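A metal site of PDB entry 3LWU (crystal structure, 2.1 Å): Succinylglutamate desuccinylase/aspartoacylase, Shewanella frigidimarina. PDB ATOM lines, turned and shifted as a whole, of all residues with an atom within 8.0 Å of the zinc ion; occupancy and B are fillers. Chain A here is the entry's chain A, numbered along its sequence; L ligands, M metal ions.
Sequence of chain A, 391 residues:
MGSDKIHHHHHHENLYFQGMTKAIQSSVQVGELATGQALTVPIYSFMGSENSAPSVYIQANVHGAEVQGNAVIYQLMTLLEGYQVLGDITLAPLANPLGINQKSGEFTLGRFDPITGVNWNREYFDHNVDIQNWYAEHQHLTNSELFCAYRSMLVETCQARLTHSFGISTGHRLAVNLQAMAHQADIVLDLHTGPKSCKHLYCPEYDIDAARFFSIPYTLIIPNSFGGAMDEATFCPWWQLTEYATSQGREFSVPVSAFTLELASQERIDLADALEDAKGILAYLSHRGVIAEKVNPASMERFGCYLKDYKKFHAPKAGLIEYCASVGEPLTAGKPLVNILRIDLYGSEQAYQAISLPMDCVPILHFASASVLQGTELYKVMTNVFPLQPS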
ATOM      1  N   ASN A  61      18.216 -23.400 -25.892  1.00  0.00           N
ATOM      2  CA  ASN A  61      18.113 -24.373 -27.011  1.00  0.00           C
ATOM      3  C   ASN A  61      18.322 -25.806 -26.562  1.00  0.00           C
ATOM      4  O   ASN A  61      18.702 -26.666 -27.335  1.00  0.00           O
ATOM      5  CB  ASN A  61      19.090 -23.973 -28.133  1.00  0.00           C
ATOM      6  CG  ASN A  61      18.690 -24.452 -29.558  1.00  0.00           C
ATOM      7  OD1 ASN A  61      19.433 -24.176 -30.493  1.00  0.00           O
ATOM      8  ND2 ASN A  61      17.529 -25.127 -29.729  1.00  0.00           N
ATOM      9  N   VAL A  62      18.007 -26.083 -25.286  1.00  0.00           N
ATOM     10  CA  VAL A  62      17.989 -27.463 -24.809  1.00  0.00           C
ATOM     11  C   VAL A  62      16.948 -28.294 -25.563  1.00  0.00           C
ATOM     12  O   VAL A  62      17.147 -29.493 -25.816  1.00  0.00           O
ATOM     13  CB  VAL A  62      17.737 -27.538 -23.316  1.00  0.00           C
ATOM     14  CG1 VAL A  62      17.444 -28.964 -22.896  1.00  0.00           C
ATOM     15  CG2 VAL A  62      18.969 -26.994 -22.578  1.00  0.00           C
ATOM     16  N   HIS A  63      15.840 -27.661 -25.877  1.00  0.00           N
ATOM     17  CA  HIS A  63      14.870 -28.211 -26.821  1.00  0.00           C
ATOM     18  C   HIS A  63      15.347 -27.749 -28.167  1.00  0.00           C
ATOM     19  O   HIS A  63      15.406 -26.565 -28.406  1.00  0.00           O
ATOM     20  CB  HIS A  63      13.439 -27.689 -26.498  1.00  0.00           C
ATOM     21  CG  HIS A  63      12.788 -28.411 -25.356  1.00  0.00           C
ATOM     22  ND1 HIS A  63      12.009 -27.776 -24.412  1.00  0.00           N
ATOM     23  CD2 HIS A  63      12.862 -29.705 -24.967  1.00  0.00           C
ATOM     24  CE1 HIS A  63      11.581 -28.649 -23.519  1.00  0.00           C
ATOM     25  NE2 HIS A  63      12.095 -29.831 -23.829  1.00  0.00           N
ATOM     26  N   GLY A  64      15.681 -28.659 -29.079  1.00  0.00           N
ATOM     27  CA  GLY A  64      16.470 -28.285 -30.243  1.00  0.00           C
ATOM     28  C   GLY A  64      15.806 -27.437 -31.299  1.00  0.00           C
ATOM     29  O   GLY A  64      16.495 -26.805 -32.085  1.00  0.00           O
ATOM     30  N   ALA A  65      14.470 -27.438 -31.335  1.00  0.00           N
ATOM     31  CA  ALA A  65      13.711 -26.599 -32.255  1.00  0.00           C
ATOM     32  C   ALA A  65      13.608 -25.175 -31.770  1.00  0.00           C
ATOM     33  O   ALA A  65      13.234 -24.262 -32.512  1.00  0.00           O
ATOM     34  CB  ALA A  65      12.237 -27.179 -32.425  1.00  0.00           C
ATOM     35  N   GLU A  66      13.908 -24.978 -30.494  1.00  0.00           N
ATOM     36  CA  GLU A  66      13.680 -23.707 -29.831  1.00  0.00           C
ATOM     37  C   GLU A  66      14.905 -22.828 -29.972  1.00  0.00           C
ATOM     38  O   GLU A  66      15.632 -22.611 -28.986  1.00  0.00           O
ATOM     39  CB  GLU A  66      13.270 -23.978 -28.390  1.00  0.00           C
ATOM     40  CG  GLU A  66      11.967 -24.762 -28.307  1.00  0.00           C
ATOM     41  CD  GLU A  66      11.503 -25.130 -26.912  1.00  0.00           C
ATOM     42  OE1 GLU A  66      12.093 -24.611 -25.942  1.00  0.00           O
ATOM     43  OE2 GLU A  66      10.579 -26.013 -26.769  1.00  0.00           O
ATOM     44  N   GLY A 110      13.630 -31.995 -31.857  1.00  0.00           N
ATOM     45  CA  GLY A 110      14.564 -31.597 -30.821  1.00  0.00           C
ATOM     46  C   GLY A 110      14.095 -31.690 -29.407  1.00  0.00           C
ATOM     47  O   GLY A 110      14.822 -31.321 -28.489  1.00  0.00           O
ATOM     48  N   ARG A 111      12.874 -32.158 -29.201  1.00  0.00           N
ATOM     49  CA  ARG A 111      12.270 -32.094 -27.888  1.00  0.00           C
ATOM     50  C   ARG A 111      12.672 -33.234 -26.959  1.00  0.00           C
ATOM     51  O   ARG A 111      12.769 -33.056 -25.718  1.00  0.00           O
ATOM     52  CB  ARG A 111      10.753 -32.073 -28.048  1.00  0.00           C
ATOM     53  CG  ARG A 111      10.004 -31.932 -26.744  1.00  0.00           C
ATOM     54  CD  ARG A 111       8.506 -31.929 -27.042  1.00  0.00           C
ATOM     55  NE  ARG A 111       7.729 -31.691 -25.838  1.00  0.00           N
ATOM     56  CZ  ARG A 111       7.646 -30.502 -25.228  1.00  0.00           C
ATOM     57  NH1 ARG A 111       8.289 -29.453 -25.723  1.00  0.00           N
ATOM     58  NH2 ARG A 111       6.945 -30.384 -24.097  1.00  0.00           N
ATOM     59  N   ASN A 119      11.962 -36.517 -22.678  1.00  0.00           N
ATOM     60  CA  ASN A 119      12.021 -35.093 -22.845  1.00  0.00           C
ATOM     61  C   ASN A 119      13.336 -34.576 -22.234  1.00  0.00           C
ATOM     62  O   ASN A 119      13.623 -34.853 -21.094  1.00  0.00           O
ATOM     63  CB  ASN A 119      10.812 -34.468 -22.140  1.00  0.00           C
ATOM     64  CG  ASN A 119      10.654 -32.935 -22.400  1.00  0.00           C
ATOM     65  OD1 ASN A 119      11.638 -32.181 -22.437  1.00  0.00           O
ATOM     66  ND2 ASN A 119       9.388 -32.491 -22.583  1.00  0.00           N
ATOM     67  N   ASN A 121      14.167 -31.738 -21.270  1.00  0.00           N
ATOM     68  CA  ASN A 121      13.916 -30.862 -20.139  1.00  0.00           C
ATOM     69  C   ASN A 121      13.274 -31.522 -18.927  1.00  0.00           C
ATOM     70  O   ASN A 121      12.805 -30.806 -18.022  1.00  0.00           O
ATOM     71  CB  ASN A 121      13.089 -29.645 -20.548  1.00  0.00           C
ATOM     72  CG  ASN A 121      13.289 -28.466 -19.612  1.00  0.00           C
ATOM     73  OD1 ASN A 121      14.364 -28.256 -19.032  1.00  0.00           O
ATOM     74  ND2 ASN A 121      12.225 -27.705 -19.425  1.00  0.00           N
ATOM     75  N   ASP A 190      16.902 -19.992 -18.167  1.00  0.00           N
ATOM     76  CA  ASP A 190      16.802 -21.059 -19.170  1.00  0.00           C
ATOM     77  C   ASP A 190      15.896 -20.541 -20.266  1.00  0.00           C
ATOM     78  O   ASP A 190      14.729 -20.298 -20.027  1.00  0.00           O
ATOM     79  CB  ASP A 190      16.211 -22.320 -18.535  1.00  0.00           C
ATOM     80  CG  ASP A 190      16.352 -23.557 -19.397  1.00  0.00           C
ATOM     81  OD1 ASP A 190      17.047 -23.519 -20.434  1.00  0.00           O
ATOM     82  OD2 ASP A 190      15.727 -24.601 -19.021  1.00  0.00           O
ATOM     83  N   LEU A 191      16.450 -20.344 -21.446  1.00  0.00           N
ATOM     84  CA  LEU A 191      15.737 -19.752 -22.562  1.00  0.00           C
ATOM     85  C   LEU A 191      15.169 -20.793 -23.518  1.00  0.00           C
ATOM     86  O   LEU A 191      15.898 -21.553 -24.151  1.00  0.00           O
ATOM     87  CB  LEU A 191      16.682 -18.842 -23.353  1.00  0.00           C
ATOM     88  CG  LEU A 191      17.453 -17.755 -22.617  1.00  0.00           C
ATOM     89  CD1 LEU A 191      18.127 -16.871 -23.599  1.00  0.00           C
ATOM     90  CD2 LEU A 191      16.564 -16.902 -21.671  1.00  0.00           C
ATOM     91  N   HIS A 192      13.847 -20.774 -23.622  1.00  0.00           N
ATOM     92  CA  HIS A 192      13.056 -21.684 -24.420  1.00  0.00           C
ATOM     93  C   HIS A 192      12.163 -20.895 -25.393  1.00  0.00           C
ATOM     94  O   HIS A 192      12.168 -19.687 -25.418  1.00  0.00           O
ATOM     95  CB  HIS A 192      12.183 -22.524 -23.496  1.00  0.00           C
ATOM     96  CG  HIS A 192      12.930 -23.586 -22.742  1.00  0.00           C
ATOM     97  ND1 HIS A 192      12.760 -24.929 -22.985  1.00  0.00           N
ATOM     98  CD2 HIS A 192      13.799 -23.495 -21.696  1.00  0.00           C
ATOM     99  CE1 HIS A 192      13.474 -25.619 -22.119  1.00  0.00           C
ATOM    100  NE2 HIS A 192      14.132 -24.778 -21.343  1.00  0.00           N
ATOM    101  N   THR A 193      11.447 -21.617 -26.265  1.00  0.00           N
ATOM    102  CA  THR A 193      10.326 -21.052 -27.006  1.00  0.00           C
ATOM    103  C   THR A 193       9.156 -22.011 -26.893  1.00  0.00           C
ATOM    104  O   THR A 193       9.334 -23.180 -26.562  1.00  0.00           O
ATOM    105  CB  THR A 193      10.613 -20.852 -28.528  1.00  0.00           C
ATOM    106  OG1 THR A 193      10.417 -22.099 -29.206  1.00  0.00           O
ATOM    107  CG2 THR A 193      12.029 -20.293 -28.805  1.00  0.00           C
ATOM    108  N   GLY A 194       7.964 -21.534 -27.206  1.00  0.00           N
ATOM    109  CA  GLY A 194       6.817 -22.414 -27.346  1.00  0.00           C
ATOM    110  C   GLY A 194       6.758 -22.843 -28.794  1.00  0.00           C
ATOM    111  O   GLY A 194       7.706 -22.627 -29.538  1.00  0.00           O
ATOM    112  N   PRO A 195       5.665 -23.486 -29.188  1.00  0.00           N
ATOM    113  CA  PRO A 195       5.538 -23.923 -30.597  1.00  0.00           C
ATOM    114  C   PRO A 195       5.110 -22.780 -31.510  1.00  0.00           C
ATOM    115  O   PRO A 195       5.986 -22.123 -32.050  1.00  0.00           O
ATOM    116  CB  PRO A 195       4.557 -25.097 -30.523  1.00  0.00           C
ATOM    117  CG  PRO A 195       3.795 -24.852 -29.296  1.00  0.00           C
ATOM    118  CD  PRO A 195       4.730 -24.193 -28.311  1.00  0.00           C
ATOM    119  N   TYR A 202       8.007 -18.554 -16.894  1.00  0.00           N
ATOM    120  CA  TYR A 202       7.737 -19.412 -15.750  1.00  0.00           C
ATOM    121  C   TYR A 202       8.518 -18.821 -14.596  1.00  0.00           C
ATOM    122  O   TYR A 202       9.746 -18.700 -14.687  1.00  0.00           O
ATOM    123  CB  TYR A 202       8.245 -20.805 -16.022  1.00  0.00           C
ATOM    124  CG  TYR A 202       7.330 -21.654 -16.854  1.00  0.00           C
ATOM    125  CD1 TYR A 202       7.431 -21.661 -18.229  1.00  0.00           C
ATOM    126  CD2 TYR A 202       6.360 -22.456 -16.275  1.00  0.00           C
ATOM    127  CE1 TYR A 202       6.626 -22.447 -19.013  1.00  0.00           C
ATOM    128  CE2 TYR A 202       5.527 -23.251 -17.064  1.00  0.00           C
ATOM    129  CZ  TYR A 202       5.664 -23.213 -18.433  1.00  0.00           C
ATOM    130  OH  TYR A 202       4.885 -23.994 -19.254  1.00  0.00           O
ATOM    131  N   THR A 260      12.384 -19.673 -16.404  1.00  0.00           N
ATOM    132  CA  THR A 260      12.343 -20.216 -17.783  1.00  0.00           C
ATOM    133  C   THR A 260      11.590 -19.187 -18.628  1.00  0.00           C
ATOM    134  O   THR A 260      10.410 -18.861 -18.364  1.00  0.00           O
ATOM    135  CB  THR A 260      11.646 -21.583 -17.844  1.00  0.00           C
ATOM    136  OG1 THR A 260      12.348 -22.524 -17.011  1.00  0.00           O
ATOM    137  CG2 THR A 260      11.489 -22.170 -19.273  1.00  0.00           C
ATOM    138  N   LEU A 261      12.298 -18.632 -19.621  1.00  0.00           N
ATOM    139  CA  LEU A 261      11.696 -17.688 -20.548  1.00  0.00           C
ATOM    140  C   LEU A 261      11.221 -18.429 -21.804  1.00  0.00           C
ATOM    141  O   LEU A 261      11.921 -19.283 -22.317  1.00  0.00           O
ATOM    142  CB  LEU A 261      12.704 -16.622 -20.948  1.00  0.00           C
ATOM    143  CG  LEU A 261      12.983 -15.524 -19.924  1.00  0.00           C
ATOM    144  CD1 LEU A 261      13.482 -16.107 -18.633  1.00  0.00           C
ATOM    145  CD2 LEU A 261      13.964 -14.499 -20.531  1.00  0.00           C
ATOM    146  N   GLU A 262      10.018 -18.129 -22.254  1.00  0.00           N
ATOM    147  CA  GLU A 262       9.468 -18.734 -23.477  1.00  0.00           C
ATOM    148  C   GLU A 262       9.349 -17.638 -24.527  1.00  0.00           C
ATOM    149  O   GLU A 262       8.405 -16.855 -24.533  1.00  0.00           O
ATOM    150  CB  GLU A 262       8.125 -19.391 -23.163  1.00  0.00           C
ATOM    151  CG  GLU A 262       8.165 -20.376 -22.000  1.00  0.00           C
ATOM    152  CD  GLU A 262       8.802 -21.701 -22.353  1.00  0.00           C
ATOM    153  OE1 GLU A 262       8.809 -22.095 -23.567  1.00  0.00           O
ATOM    154  OE2 GLU A 262       9.241 -22.381 -21.405  1.00  0.00           O
ATOM    155  N   GLN A 266       8.958 -21.487 -31.839  1.00  0.00           N
ATOM    156  CA  GLN A 266      10.067 -22.344 -32.288  1.00  0.00           C
ATOM    157  C   GLN A 266      10.357 -22.201 -33.767  1.00  0.00           C
ATOM    158  O   GLN A 266       9.601 -21.545 -34.507  1.00  0.00           O
ATOM    159  CB  GLN A 266       9.737 -23.802 -31.965  1.00  0.00           C
ATOM    160  CG  GLN A 266       8.622 -24.372 -32.834  1.00  0.00           C
ATOM    161  CD  GLN A 266       8.177 -25.750 -32.372  1.00  0.00           C
ATOM    162  OE1 GLN A 266       8.559 -26.204 -31.300  1.00  0.00           O
ATOM    163  NE2 GLN A 266       7.307 -26.402 -33.183  1.00  0.00           N
HETATM  164  O1  LIG L   1       6.979 -27.447 -23.473  1.00  0.00           O
HETATM  165  O2  LIG L   1       7.543 -26.116 -23.962  1.00  0.00           O
HETATM  166  O3  LIG L   1       6.503 -24.965 -23.979  1.00  0.00           O
HETATM  167  O4  LIG L   1       5.178 -25.273 -23.096  1.00  0.00           O
HETATM  168  O5  LIG L   1       4.630 -23.956 -22.483  1.00  0.00           O
HETATM  169  O6  LIG L   1       5.346 -22.902 -22.650  1.00  0.00           O
HETATM  170  O7  LIG L   1       3.531 -23.982 -21.885  1.00  0.00           O
HETATM  171  O8  LIG L   1       8.926 -25.555 -23.463  1.00  0.00           O
HETATM  172  O9  LIG L   1       9.625 -25.296 -24.415  1.00  0.00           O
HETATM  173  O10 LIG L   1       9.367 -25.254 -22.359  1.00  0.00           O
HETATM  174  O11 LIG L   1       8.443 -25.390 -26.229  1.00  0.00           O
HETATM  175  O12 LIG L   1       7.650 -25.738 -28.096  1.00  0.00           O
HETATM  176 ZN    ZN M   1      11.479 -25.765 -24.360  1.00  0.00          ZN
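Of the 21 residues printed, 3 come within 4 Å of the zinc ion.
The side-chain carboxylate (OE1) of Glu 66 sits close to the backbone NH (N) of Thr 193 (3.1 Å).
The backbone carbonyl oxygen of Glu 66 lies within hydrogen-bond range of the side-chain amide nitrogen of Asn 61 (3.2 Å).
The backbone NH (N) of His 192 is in hydrogen-bond range of the backbone carbonyl oxygen (O) of Leu 261 (2.8 Å).
A ring nitrogen (NE2) of His 192 is in hydrogen-bond range of the side-chain carboxylate (OD2) of Asp 190 (2.8 Å).
A ring nitrogen (NE2) of His 63 lies within hydrogen-bond range of the side-chain amide oxygen (OD1) of Asn 119 (2.8 Å).
O of His 63 sits at hydrogen-bond distance from ND2 of Asn 61 (2.9 Å).
The zinc ion is bound by an oxygen (O9) of the ligand (1.9 Å).
OE1 of Glu 66 binds the zinc ion (2.1 Å).
The zinc ion is bound by a ring nitrogen (ND1) of His 192 (2.1 Å).
The zinc ion is bound by ND1 of His 63.
OE2 of Glu 66 binds the zinc ion (2.6 Å).
The zinc ion has five donor atoms within binding distance.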
